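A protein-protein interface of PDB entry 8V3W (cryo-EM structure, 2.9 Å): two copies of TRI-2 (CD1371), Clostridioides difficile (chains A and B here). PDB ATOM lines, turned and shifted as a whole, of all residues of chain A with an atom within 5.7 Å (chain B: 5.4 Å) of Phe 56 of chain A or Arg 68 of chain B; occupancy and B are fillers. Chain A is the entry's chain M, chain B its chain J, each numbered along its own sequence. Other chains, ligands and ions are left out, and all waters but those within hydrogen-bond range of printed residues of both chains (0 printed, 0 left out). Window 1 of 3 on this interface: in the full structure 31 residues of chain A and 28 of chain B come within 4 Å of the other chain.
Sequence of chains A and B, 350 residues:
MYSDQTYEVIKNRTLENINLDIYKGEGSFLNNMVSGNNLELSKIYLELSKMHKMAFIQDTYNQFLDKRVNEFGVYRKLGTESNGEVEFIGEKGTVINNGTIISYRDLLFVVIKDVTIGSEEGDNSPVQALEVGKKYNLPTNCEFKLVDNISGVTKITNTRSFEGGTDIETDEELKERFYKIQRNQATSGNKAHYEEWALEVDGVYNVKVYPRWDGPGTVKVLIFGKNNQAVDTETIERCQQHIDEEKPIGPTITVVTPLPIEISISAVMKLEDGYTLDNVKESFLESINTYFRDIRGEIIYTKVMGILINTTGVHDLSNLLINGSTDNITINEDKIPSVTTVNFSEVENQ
OE2 of Glu 71 of chain B lies within salt-bridge range of NH2 of Arg 68 of chain A, at 3.7 Å.
The backbone carbonyl oxygen of Ala 55 of chain B lies within hydrogen-bond range of the guanidinium group of Arg 68 of chain B, at 3.2 Å.
The guanidinium group of Arg 68 of chain B is in salt-bridge range of the side-chain carboxylate of Glu 71 of chain B (3.6 Å).
The backbone carbonyl oxygen (O) of Ala 55 of chain A is in hydrogen-bond range of the guanidinium group (NH1) of Arg 68 of chain A.
Among the printed residues, pairs that only touch across the chains: His 52 of chain A with Ala 55 of chain B (3.6 Å), His 52 of chain A with Phe 64 of chain B (3.1 Å), Phe 56 of chain A with Phe 64 of chain B (3.3 Å), Phe 56 of chain A with Lys 67 of chain B (3.5 Å), Phe 56 of chain A with Arg 68 of chain B (3.7 Å), Ile 57 of chain A with Glu 71 of chain B (3.2 Å) and Gln 58 of chain A with Lys 67 of chain B (3.3 Å).
Of chain B, only Phe 64 (3.3 Å), Lys 67 (3.5 Å) and Arg 68 (3.7 Å) come within 4 Å of Phe 56 of chain A.
Printed residues of chain A within 4 Å of Phe 64 of chain B: His 52 (3.1 Å) and Phe 56 (3.3 Å).
Of the printed residues of chain B, His 52 of chain A touches Ala 55 (3.6 Å) and Phe 64 (3.1 Å).
Of the printed residues of chain B, Arg 68 of chain A touches Glu 71 (3.7 Å).
Printed residues of chain B within 4 Å of Ile 57 of chain A: Glu 71 (3.2 Å).
Val 69 of chain B touches none of the printed residues of chain A.
The nearest residue of chain B that does not touch Phe 56 of chain A is Glu 71 of chain B (4.6 Å).
The nearest residue of chain A that does not touch Arg 68 of chain B is Arg 68 of chain A (4.8 Å).
The nearest printed residue of chain B that does not touch Arg 68 of chain A is Arg 68 of chain B (4.8 Å).
Of the 11 printed residues of chain A, 5 touch a printed residue of chain B.
Printed residues of chain A that touch a printed residue of chain B: His 52, Phe 56, Ile 57, Gln 58 and Arg 68.
Printed residues of chain B that touch a printed residue of chain A: Ala 55, Phe 64, Lys 67, Arg 68 and Glu 71.
Among the printed residues, Asp or Glu carboxylates within 4 Å of a Lys or Arg side-chain nitrogen of the other chain: Arg 68 of chain A with Glu 71 of chain B (3.7 Å).
Phe 56 of chain A touches Arg 68 of chain B, but with the chains exchanged Arg 68 of chain A does not touch Phe 56 of chain B (7.9 Å).
Positions printed for both chains: 55, 56, 57 and 68.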
ATOM      1  N   MET A  51       4.557 -14.578  10.327  1.00  0.00           N
ATOM      2  CA  MET A  51       4.913 -15.958  10.002  1.00  0.00           C
ATOM      3  C   MET A  51       6.318 -16.305  10.483  1.00  0.00           C
ATOM      4  O   MET A  51       6.532 -17.348  11.118  1.00  0.00           O
ATOM      5  CB  MET A  51       4.786 -16.180   8.496  1.00  0.00           C
ATOM      6  CG  MET A  51       3.420 -16.686   8.059  1.00  0.00           C
ATOM      7  SD  MET A  51       3.518 -17.857   6.695  1.00  0.00           S
ATOM      8  CE  MET A  51       4.813 -17.110   5.711  1.00  0.00           C
ATOM      9  N   HIS A  52       7.291 -15.437  10.201  1.00  0.00           N
ATOM     10  CA  HIS A  52       8.662 -15.746  10.584  1.00  0.00           C
ATOM     11  C   HIS A  52       8.824 -15.770  12.096  1.00  0.00           C
ATOM     12  O   HIS A  52       9.680 -16.494  12.614  1.00  0.00           O
ATOM     13  CB  HIS A  52       9.638 -14.747   9.966  1.00  0.00           C
ATOM     14  CG  HIS A  52      10.434 -15.313   8.833  1.00  0.00           C
ATOM     15  ND1 HIS A  52      11.614 -15.999   9.018  1.00  0.00           N
ATOM     16  CD2 HIS A  52      10.231 -15.271   7.496  1.00  0.00           C
ATOM     17  CE1 HIS A  52      12.089 -16.378   7.844  1.00  0.00           C
ATOM     18  NE2 HIS A  52      11.272 -15.943   6.904  1.00  0.00           N
ATOM     19  N   LYS A  53       8.020 -14.986  12.816  1.00  0.00           N
ATOM     20  CA  LYS A  53       8.029 -15.081  14.271  1.00  0.00           C
ATOM     21  C   LYS A  53       7.514 -16.436  14.733  1.00  0.00           C
ATOM     22  O   LYS A  53       8.144 -17.091  15.570  1.00  0.00           O
ATOM     23  CB  LYS A  53       7.212 -13.949  14.891  1.00  0.00           C
ATOM     24  CG  LYS A  53       7.991 -12.656  15.050  1.00  0.00           C
ATOM     25  CD  LYS A  53       9.398 -12.937  15.557  1.00  0.00           C
ATOM     26  CE  LYS A  53       9.805 -11.971  16.654  1.00  0.00           C
ATOM     27  NZ  LYS A  53       9.325 -12.435  17.985  1.00  0.00           N
ATOM     28  N   MET A  54       6.381 -16.892  14.192  1.00  0.00           N
ATOM     29  CA  MET A  54       5.913 -18.187  14.685  1.00  0.00           C
ATOM     30  C   MET A  54       6.693 -19.363  14.111  1.00  0.00           C
ATOM     31  O   MET A  54       6.419 -20.505  14.493  1.00  0.00           O
ATOM     32  CB  MET A  54       4.415 -18.439  14.442  1.00  0.00           C
ATOM     33  CG  MET A  54       3.902 -18.471  13.009  1.00  0.00           C
ATOM     34  SD  MET A  54       2.149 -18.012  12.968  1.00  0.00           S
ATOM     35  CE  MET A  54       2.136 -16.450  12.113  1.00  0.00           C
ATOM     36  N   ALA A  55       7.644 -19.124  13.204  1.00  0.00           N
ATOM     37  CA  ALA A  55       8.433 -20.232  12.667  1.00  0.00           C
ATOM     38  C   ALA A  55       9.459 -20.754  13.674  1.00  0.00           C
ATOM     39  O   ALA A  55       9.662 -21.970  13.781  1.00  0.00           O
ATOM     40  CB  ALA A  55       9.127 -19.802  11.376  1.00  0.00           C
ATOM     41  N   PHE A  56      10.111 -19.862  14.421  1.00  0.00           N
ATOM     42  CA  PHE A  56      11.286 -20.225  15.206  1.00  0.00           C
ATOM     43  C   PHE A  56      10.912 -21.073  16.422  1.00  0.00           C
ATOM     44  O   PHE A  56       9.761 -21.472  16.612  1.00  0.00           O
ATOM     45  CB  PHE A  56      12.038 -18.974  15.648  1.00  0.00           C
ATOM     46  CG  PHE A  56      12.891 -18.375  14.575  1.00  0.00           C
ATOM     47  CD1 PHE A  56      13.145 -19.075  13.407  1.00  0.00           C
ATOM     48  CD2 PHE A  56      13.443 -17.120  14.734  1.00  0.00           C
ATOM     49  CE1 PHE A  56      13.933 -18.531  12.419  1.00  0.00           C
ATOM     50  CE2 PHE A  56      14.232 -16.569  13.748  1.00  0.00           C
ATOM     51  CZ  PHE A  56      14.477 -17.276  12.589  1.00  0.00           C
ATOM     52  N   ILE A  57      11.922 -21.355  17.252  1.00  0.00           N
ATOM     53  CA  ILE A  57      11.764 -22.190  18.441  1.00  0.00           C
ATOM     54  C   ILE A  57      11.703 -21.330  19.695  1.00  0.00           C
ATOM     55  O   ILE A  57      11.094 -21.723  20.697  1.00  0.00           O
ATOM     56  CB  ILE A  57      12.895 -23.231  18.550  1.00  0.00           C
ATOM     57  CG1 ILE A  57      12.539 -24.304  19.576  1.00  0.00           C
ATOM     58  CG2 ILE A  57      14.196 -22.578  18.968  1.00  0.00           C
ATOM     59  CD1 ILE A  57      11.324 -25.099  19.230  1.00  0.00           C
ATOM     60  N   GLN A  58      12.335 -20.155  19.659  1.00  0.00           N
ATOM     61  CA  GLN A  58      12.332 -19.283  20.829  1.00  0.00           C
ATOM     62  C   GLN A  58      10.925 -18.793  21.142  1.00  0.00           C
ATOM     63  O   GLN A  58      10.549 -18.660  22.311  1.00  0.00           O
ATOM     64  CB  GLN A  58      13.275 -18.102  20.610  1.00  0.00           C
ATOM     65  CG  GLN A  58      14.747 -18.457  20.679  1.00  0.00           C
ATOM     66  CD  GLN A  58      15.311 -18.879  19.337  1.00  0.00           C
ATOM     67  OE1 GLN A  58      14.608 -19.459  18.510  1.00  0.00           O
ATOM     68  NE2 GLN A  58      16.588 -18.591  19.114  1.00  0.00           N
ATOM     69  N   ASP A  59      10.136 -18.508  20.104  1.00  0.00           N
ATOM     70  CA  ASP A  59       8.764 -18.013  20.238  1.00  0.00           C
ATOM     71  C   ASP A  59       7.892 -18.795  19.260  1.00  0.00           C
ATOM     72  O   ASP A  59       7.732 -18.401  18.104  1.00  0.00           O
ATOM     73  CB  ASP A  59       8.716 -16.521  19.975  1.00  0.00           C
ATOM     74  CG  ASP A  59       9.608 -16.112  18.821  1.00  0.00           C
ATOM     75  OD1 ASP A  59      10.842 -16.263  18.939  1.00  0.00           O
ATOM     76  OD2 ASP A  59       9.076 -15.643  17.794  1.00  0.00           O
ATOM     77  N   THR A  60       7.404 -19.957  19.692  1.00  0.00           N
ATOM     78  CA  THR A  60       6.552 -20.808  18.850  1.00  0.00           C
ATOM     79  C   THR A  60       5.120 -21.020  19.366  1.00  0.00           C
ATOM     80  O   THR A  60       4.390 -21.867  18.851  1.00  0.00           O
ATOM     81  CB  THR A  60       7.201 -22.186  18.615  1.00  0.00           C
ATOM     82  OG1 THR A  60       6.350 -22.982  17.779  1.00  0.00           O
ATOM     83  CG2 THR A  60       7.420 -22.905  19.937  1.00  0.00           C
ATOM     84  N   ARG A  68       7.599 -28.758  17.084  1.00  0.00           N
ATOM     85  CA  ARG A  68       9.048 -28.612  16.964  1.00  0.00           C
ATOM     86  C   ARG A  68       9.784 -29.470  17.994  1.00  0.00           C
ATOM     87  O   ARG A  68      10.759 -30.162  17.663  1.00  0.00           O
ATOM     88  CB  ARG A  68       9.428 -27.141  17.114  1.00  0.00           C
ATOM     89  CG  ARG A  68       8.880 -26.235  16.017  1.00  0.00           C
ATOM     90  CD  ARG A  68       9.307 -26.669  14.622  1.00  0.00           C
ATOM     91  NE  ARG A  68      10.738 -26.928  14.522  1.00  0.00           N
ATOM     92  CZ  ARG A  68      11.677 -25.995  14.608  1.00  0.00           C
ATOM     93  NH1 ARG A  68      11.375 -24.720  14.788  1.00  0.00           N
ATOM     94  NH2 ARG A  68      12.955 -26.349  14.500  1.00  0.00           N
ATOM     95  N   ALA B  55      14.779 -18.253   5.803  1.00  0.00           N
ATOM     96  CA  ALA B  55      14.372 -19.155   6.877  1.00  0.00           C
ATOM     97  C   ALA B  55      15.328 -20.335   7.015  1.00  0.00           C
ATOM     98  O   ALA B  55      15.668 -20.737   8.132  1.00  0.00           O
ATOM     99  CB  ALA B  55      12.946 -19.648   6.638  1.00  0.00           C
ATOM    100  N   PHE B  56      15.775 -20.902   5.895  1.00  0.00           N
ATOM    101  CA  PHE B  56      16.643 -22.071   5.918  1.00  0.00           C
ATOM    102  C   PHE B  56      18.112 -21.715   5.716  1.00  0.00           C
ATOM    103  O   PHE B  56      18.895 -22.577   5.305  1.00  0.00           O
ATOM    104  CB  PHE B  56      16.196 -23.083   4.863  1.00  0.00           C
ATOM    105  CG  PHE B  56      15.130 -24.021   5.342  1.00  0.00           C
ATOM    106  CD1 PHE B  56      15.400 -24.961   6.316  1.00  0.00           C
ATOM    107  CD2 PHE B  56      13.854 -23.961   4.814  1.00  0.00           C
ATOM    108  CE1 PHE B  56      14.414 -25.821   6.755  1.00  0.00           C
ATOM    109  CE2 PHE B  56      12.867 -24.819   5.248  1.00  0.00           C
ATOM    110  CZ  PHE B  56      13.146 -25.747   6.219  1.00  0.00           C
ATOM    111  N   ILE B  57      18.489 -20.465   6.006  1.00  0.00           N
ATOM    112  CA  ILE B  57      19.862 -19.953   5.980  1.00  0.00           C
ATOM    113  C   ILE B  57      20.677 -20.565   4.841  1.00  0.00           C
ATOM    114  O   ILE B  57      21.701 -21.223   5.058  1.00  0.00           O
ATOM    115  CB  ILE B  57      20.540 -20.139   7.359  1.00  0.00           C
ATOM    116  CG1 ILE B  57      21.913 -19.458   7.395  1.00  0.00           C
ATOM    117  CG2 ILE B  57      20.619 -21.609   7.792  1.00  0.00           C
ATOM    118  CD1 ILE B  57      21.905 -18.033   6.902  1.00  0.00           C
ATOM    119  N   PHE B  64      19.236 -15.326  10.412  1.00  0.00           N
ATOM    120  CA  PHE B  64      18.656 -16.440  11.143  1.00  0.00           C
ATOM    121  C   PHE B  64      19.634 -17.589  11.344  1.00  0.00           C
ATOM    122  O   PHE B  64      19.253 -18.615  11.917  1.00  0.00           O
ATOM    123  CB  PHE B  64      17.403 -16.915  10.412  1.00  0.00           C
ATOM    124  CG  PHE B  64      16.359 -15.846  10.276  1.00  0.00           C
ATOM    125  CD1 PHE B  64      16.319 -14.788  11.169  1.00  0.00           C
ATOM    126  CD2 PHE B  64      15.466 -15.859   9.225  1.00  0.00           C
ATOM    127  CE1 PHE B  64      15.377 -13.791  11.043  1.00  0.00           C
ATOM    128  CE2 PHE B  64      14.530 -14.858   9.091  1.00  0.00           C
ATOM    129  CZ  PHE B  64      14.482 -13.825  10.001  1.00  0.00           C
ATOM    130  N   LEU B  65      20.878 -17.445  10.882  1.00  0.00           N
ATOM    131  CA  LEU B  65      21.886 -18.464  11.147  1.00  0.00           C
ATOM    132  C   LEU B  65      22.192 -18.557  12.635  1.00  0.00           C
ATOM    133  O   LEU B  65      22.412 -19.652  13.164  1.00  0.00           O
ATOM    134  CB  LEU B  65      23.158 -18.172  10.348  1.00  0.00           C
ATOM    135  CG  LEU B  65      23.898 -16.850  10.566  1.00  0.00           C
ATOM    136  CD1 LEU B  65      25.046 -17.019  11.547  1.00  0.00           C
ATOM    137  CD2 LEU B  65      24.401 -16.297   9.241  1.00  0.00           C
ATOM    138  N   ASP B  66      22.213 -17.414  13.323  1.00  0.00           N
ATOM    139  CA  ASP B  66      22.528 -17.404  14.748  1.00  0.00           C
ATOM    140  C   ASP B  66      21.506 -18.208  15.540  1.00  0.00           C
ATOM    141  O   ASP B  66      21.866 -19.018  16.402  1.00  0.00           O
ATOM    142  CB  ASP B  66      22.589 -15.966  15.256  1.00  0.00           C
ATOM    143  CG  ASP B  66      23.123 -15.872  16.668  1.00  0.00           C
ATOM    144  OD1 ASP B  66      23.955 -16.723  17.045  1.00  0.00           O
ATOM    145  OD2 ASP B  66      22.708 -14.953  17.405  1.00  0.00           O
ATOM    146  N   LYS B  67      20.220 -18.008  15.251  1.00  0.00           N
ATOM    147  CA  LYS B  67      19.190 -18.735  15.982  1.00  0.00           C
ATOM    148  C   LYS B  67      19.210 -20.219  15.639  1.00  0.00           C
ATOM    149  O   LYS B  67      18.989 -21.064  16.512  1.00  0.00           O
ATOM    150  CB  LYS B  67      17.818 -18.125  15.706  1.00  0.00           C
ATOM    151  CG  LYS B  67      17.681 -16.706  16.228  1.00  0.00           C
ATOM    152  CD  LYS B  67      16.256 -16.416  16.652  1.00  0.00           C
ATOM    153  CE  LYS B  67      16.161 -15.126  17.451  1.00  0.00           C
ATOM    154  NZ  LYS B  67      14.823 -14.978  18.088  1.00  0.00           N
ATOM    155  N   ARG B  68      19.488 -20.560  14.381  1.00  0.00           N
ATOM    156  CA  ARG B  68      19.554 -21.969  14.007  1.00  0.00           C
ATOM    157  C   ARG B  68      20.727 -22.671  14.686  1.00  0.00           C
ATOM    158  O   ARG B  68      20.593 -23.811  15.150  1.00  0.00           O
ATOM    159  CB  ARG B  68      19.644 -22.103  12.488  1.00  0.00           C
ATOM    160  CG  ARG B  68      18.750 -23.192  11.918  1.00  0.00           C
ATOM    161  CD  ARG B  68      18.096 -22.756  10.618  1.00  0.00           C
ATOM    162  NE  ARG B  68      16.820 -22.082  10.822  1.00  0.00           N
ATOM    163  CZ  ARG B  68      15.672 -22.698  11.071  1.00  0.00           C
ATOM    164  NH1 ARG B  68      15.607 -24.013  11.203  1.00  0.00           N
ATOM    165  NH2 ARG B  68      14.561 -21.977  11.192  1.00  0.00           N
ATOM    166  N   VAL B  69      21.884 -22.013  14.762  1.00  0.00           N
ATOM    167  CA  VAL B  69      23.017 -22.658  15.417  1.00  0.00           C
ATOM    168  C   VAL B  69      22.845 -22.660  16.932  1.00  0.00           C
ATOM    169  O   VAL B  69      23.402 -23.524  17.618  1.00  0.00           O
ATOM    170  CB  VAL B  69      24.347 -22.007  14.999  1.00  0.00           C
ATOM    171  CG1 VAL B  69      24.574 -22.184  13.503  1.00  0.00           C
ATOM    172  CG2 VAL B  69      24.391 -20.547  15.397  1.00  0.00           C
ATOM    173  N   ASN B  70      22.088 -21.708  17.484  1.00  0.00           N
ATOM    174  CA  ASN B  70      21.700 -21.817  18.885  1.00  0.00           C
ATOM    175  C   ASN B  70      20.757 -22.992  19.100  1.00  0.00           C
ATOM    176  O   ASN B  70      20.789 -23.631  20.157  1.00  0.00           O
ATOM    177  CB  ASN B  70      21.049 -20.519  19.357  1.00  0.00           C
ATOM    178  CG  ASN B  70      22.065 -19.442  19.682  1.00  0.00           C
ATOM    179  OD1 ASN B  70      23.218 -19.509  19.252  1.00  0.00           O
ATOM    180  ND2 ASN B  70      21.644 -18.443  20.447  1.00  0.00           N
ATOM    181  N   GLU B  71      19.902 -23.274  18.116  1.00  0.00           N
ATOM    182  CA  GLU B  71      19.090 -24.484  18.155  1.00  0.00           C
ATOM    183  C   GLU B  71      19.968 -25.726  18.164  1.00  0.00           C
ATOM    184  O   GLU B  71      19.699 -26.682  18.900  1.00  0.00           O
ATOM    185  CB  GLU B  71      18.147 -24.523  16.954  1.00  0.00           C
ATOM    186  CG  GLU B  71      16.995 -23.543  17.010  1.00  0.00           C
ATOM    187  CD  GLU B  71      16.065 -23.683  15.822  1.00  0.00           C
ATOM    188  OE1 GLU B  71      16.566 -23.964  14.713  1.00  0.00           O
ATOM    189  OE2 GLU B  71      14.841 -23.513  15.991  1.00  0.00           O
ATOM    190  N   PHE B  72      21.021 -25.729  17.350  1.00  0.00           N
ATOM    191  CA  PHE B  72      21.886 -26.892  17.210  1.00  0.00           C
ATOM    192  C   PHE B  72      23.040 -26.905  18.204  1.00  0.00           C
ATOM    193  O   PHE B  72      23.894 -27.794  18.129  1.00  0.00           O
ATOM    194  CB  PHE B  72      22.422 -26.974  15.779  1.00  0.00           C
ATOM    195  CG  PHE B  72      21.446 -27.571  14.810  1.00  0.00           C
ATOM    196  CD1 PHE B  72      20.541 -26.768  14.139  1.00  0.00           C
ATOM    197  CD2 PHE B  72      21.416 -28.936  14.586  1.00  0.00           C
ATOM    198  CE1 PHE B  72      19.632 -27.314  13.255  1.00  0.00           C
ATOM    199  CE2 PHE B  72      20.512 -29.487  13.703  1.00  0.00           C
ATOM    200  CZ  PHE B  72      19.618 -28.676  13.037  1.00  0.00           C
ATOM    201  N   GLY B  73      23.094 -25.944  19.125  1.00  0.00           N
ATOM    202  CA  GLY B  73      24.087 -25.936  20.178  1.00  0.00           C
ATOM    203  C   GLY B  73      25.355 -25.169  19.869  1.00  0.00           C
ATOM    204  O   GLY B  73      26.143 -24.916  20.788  1.00  0.00           O
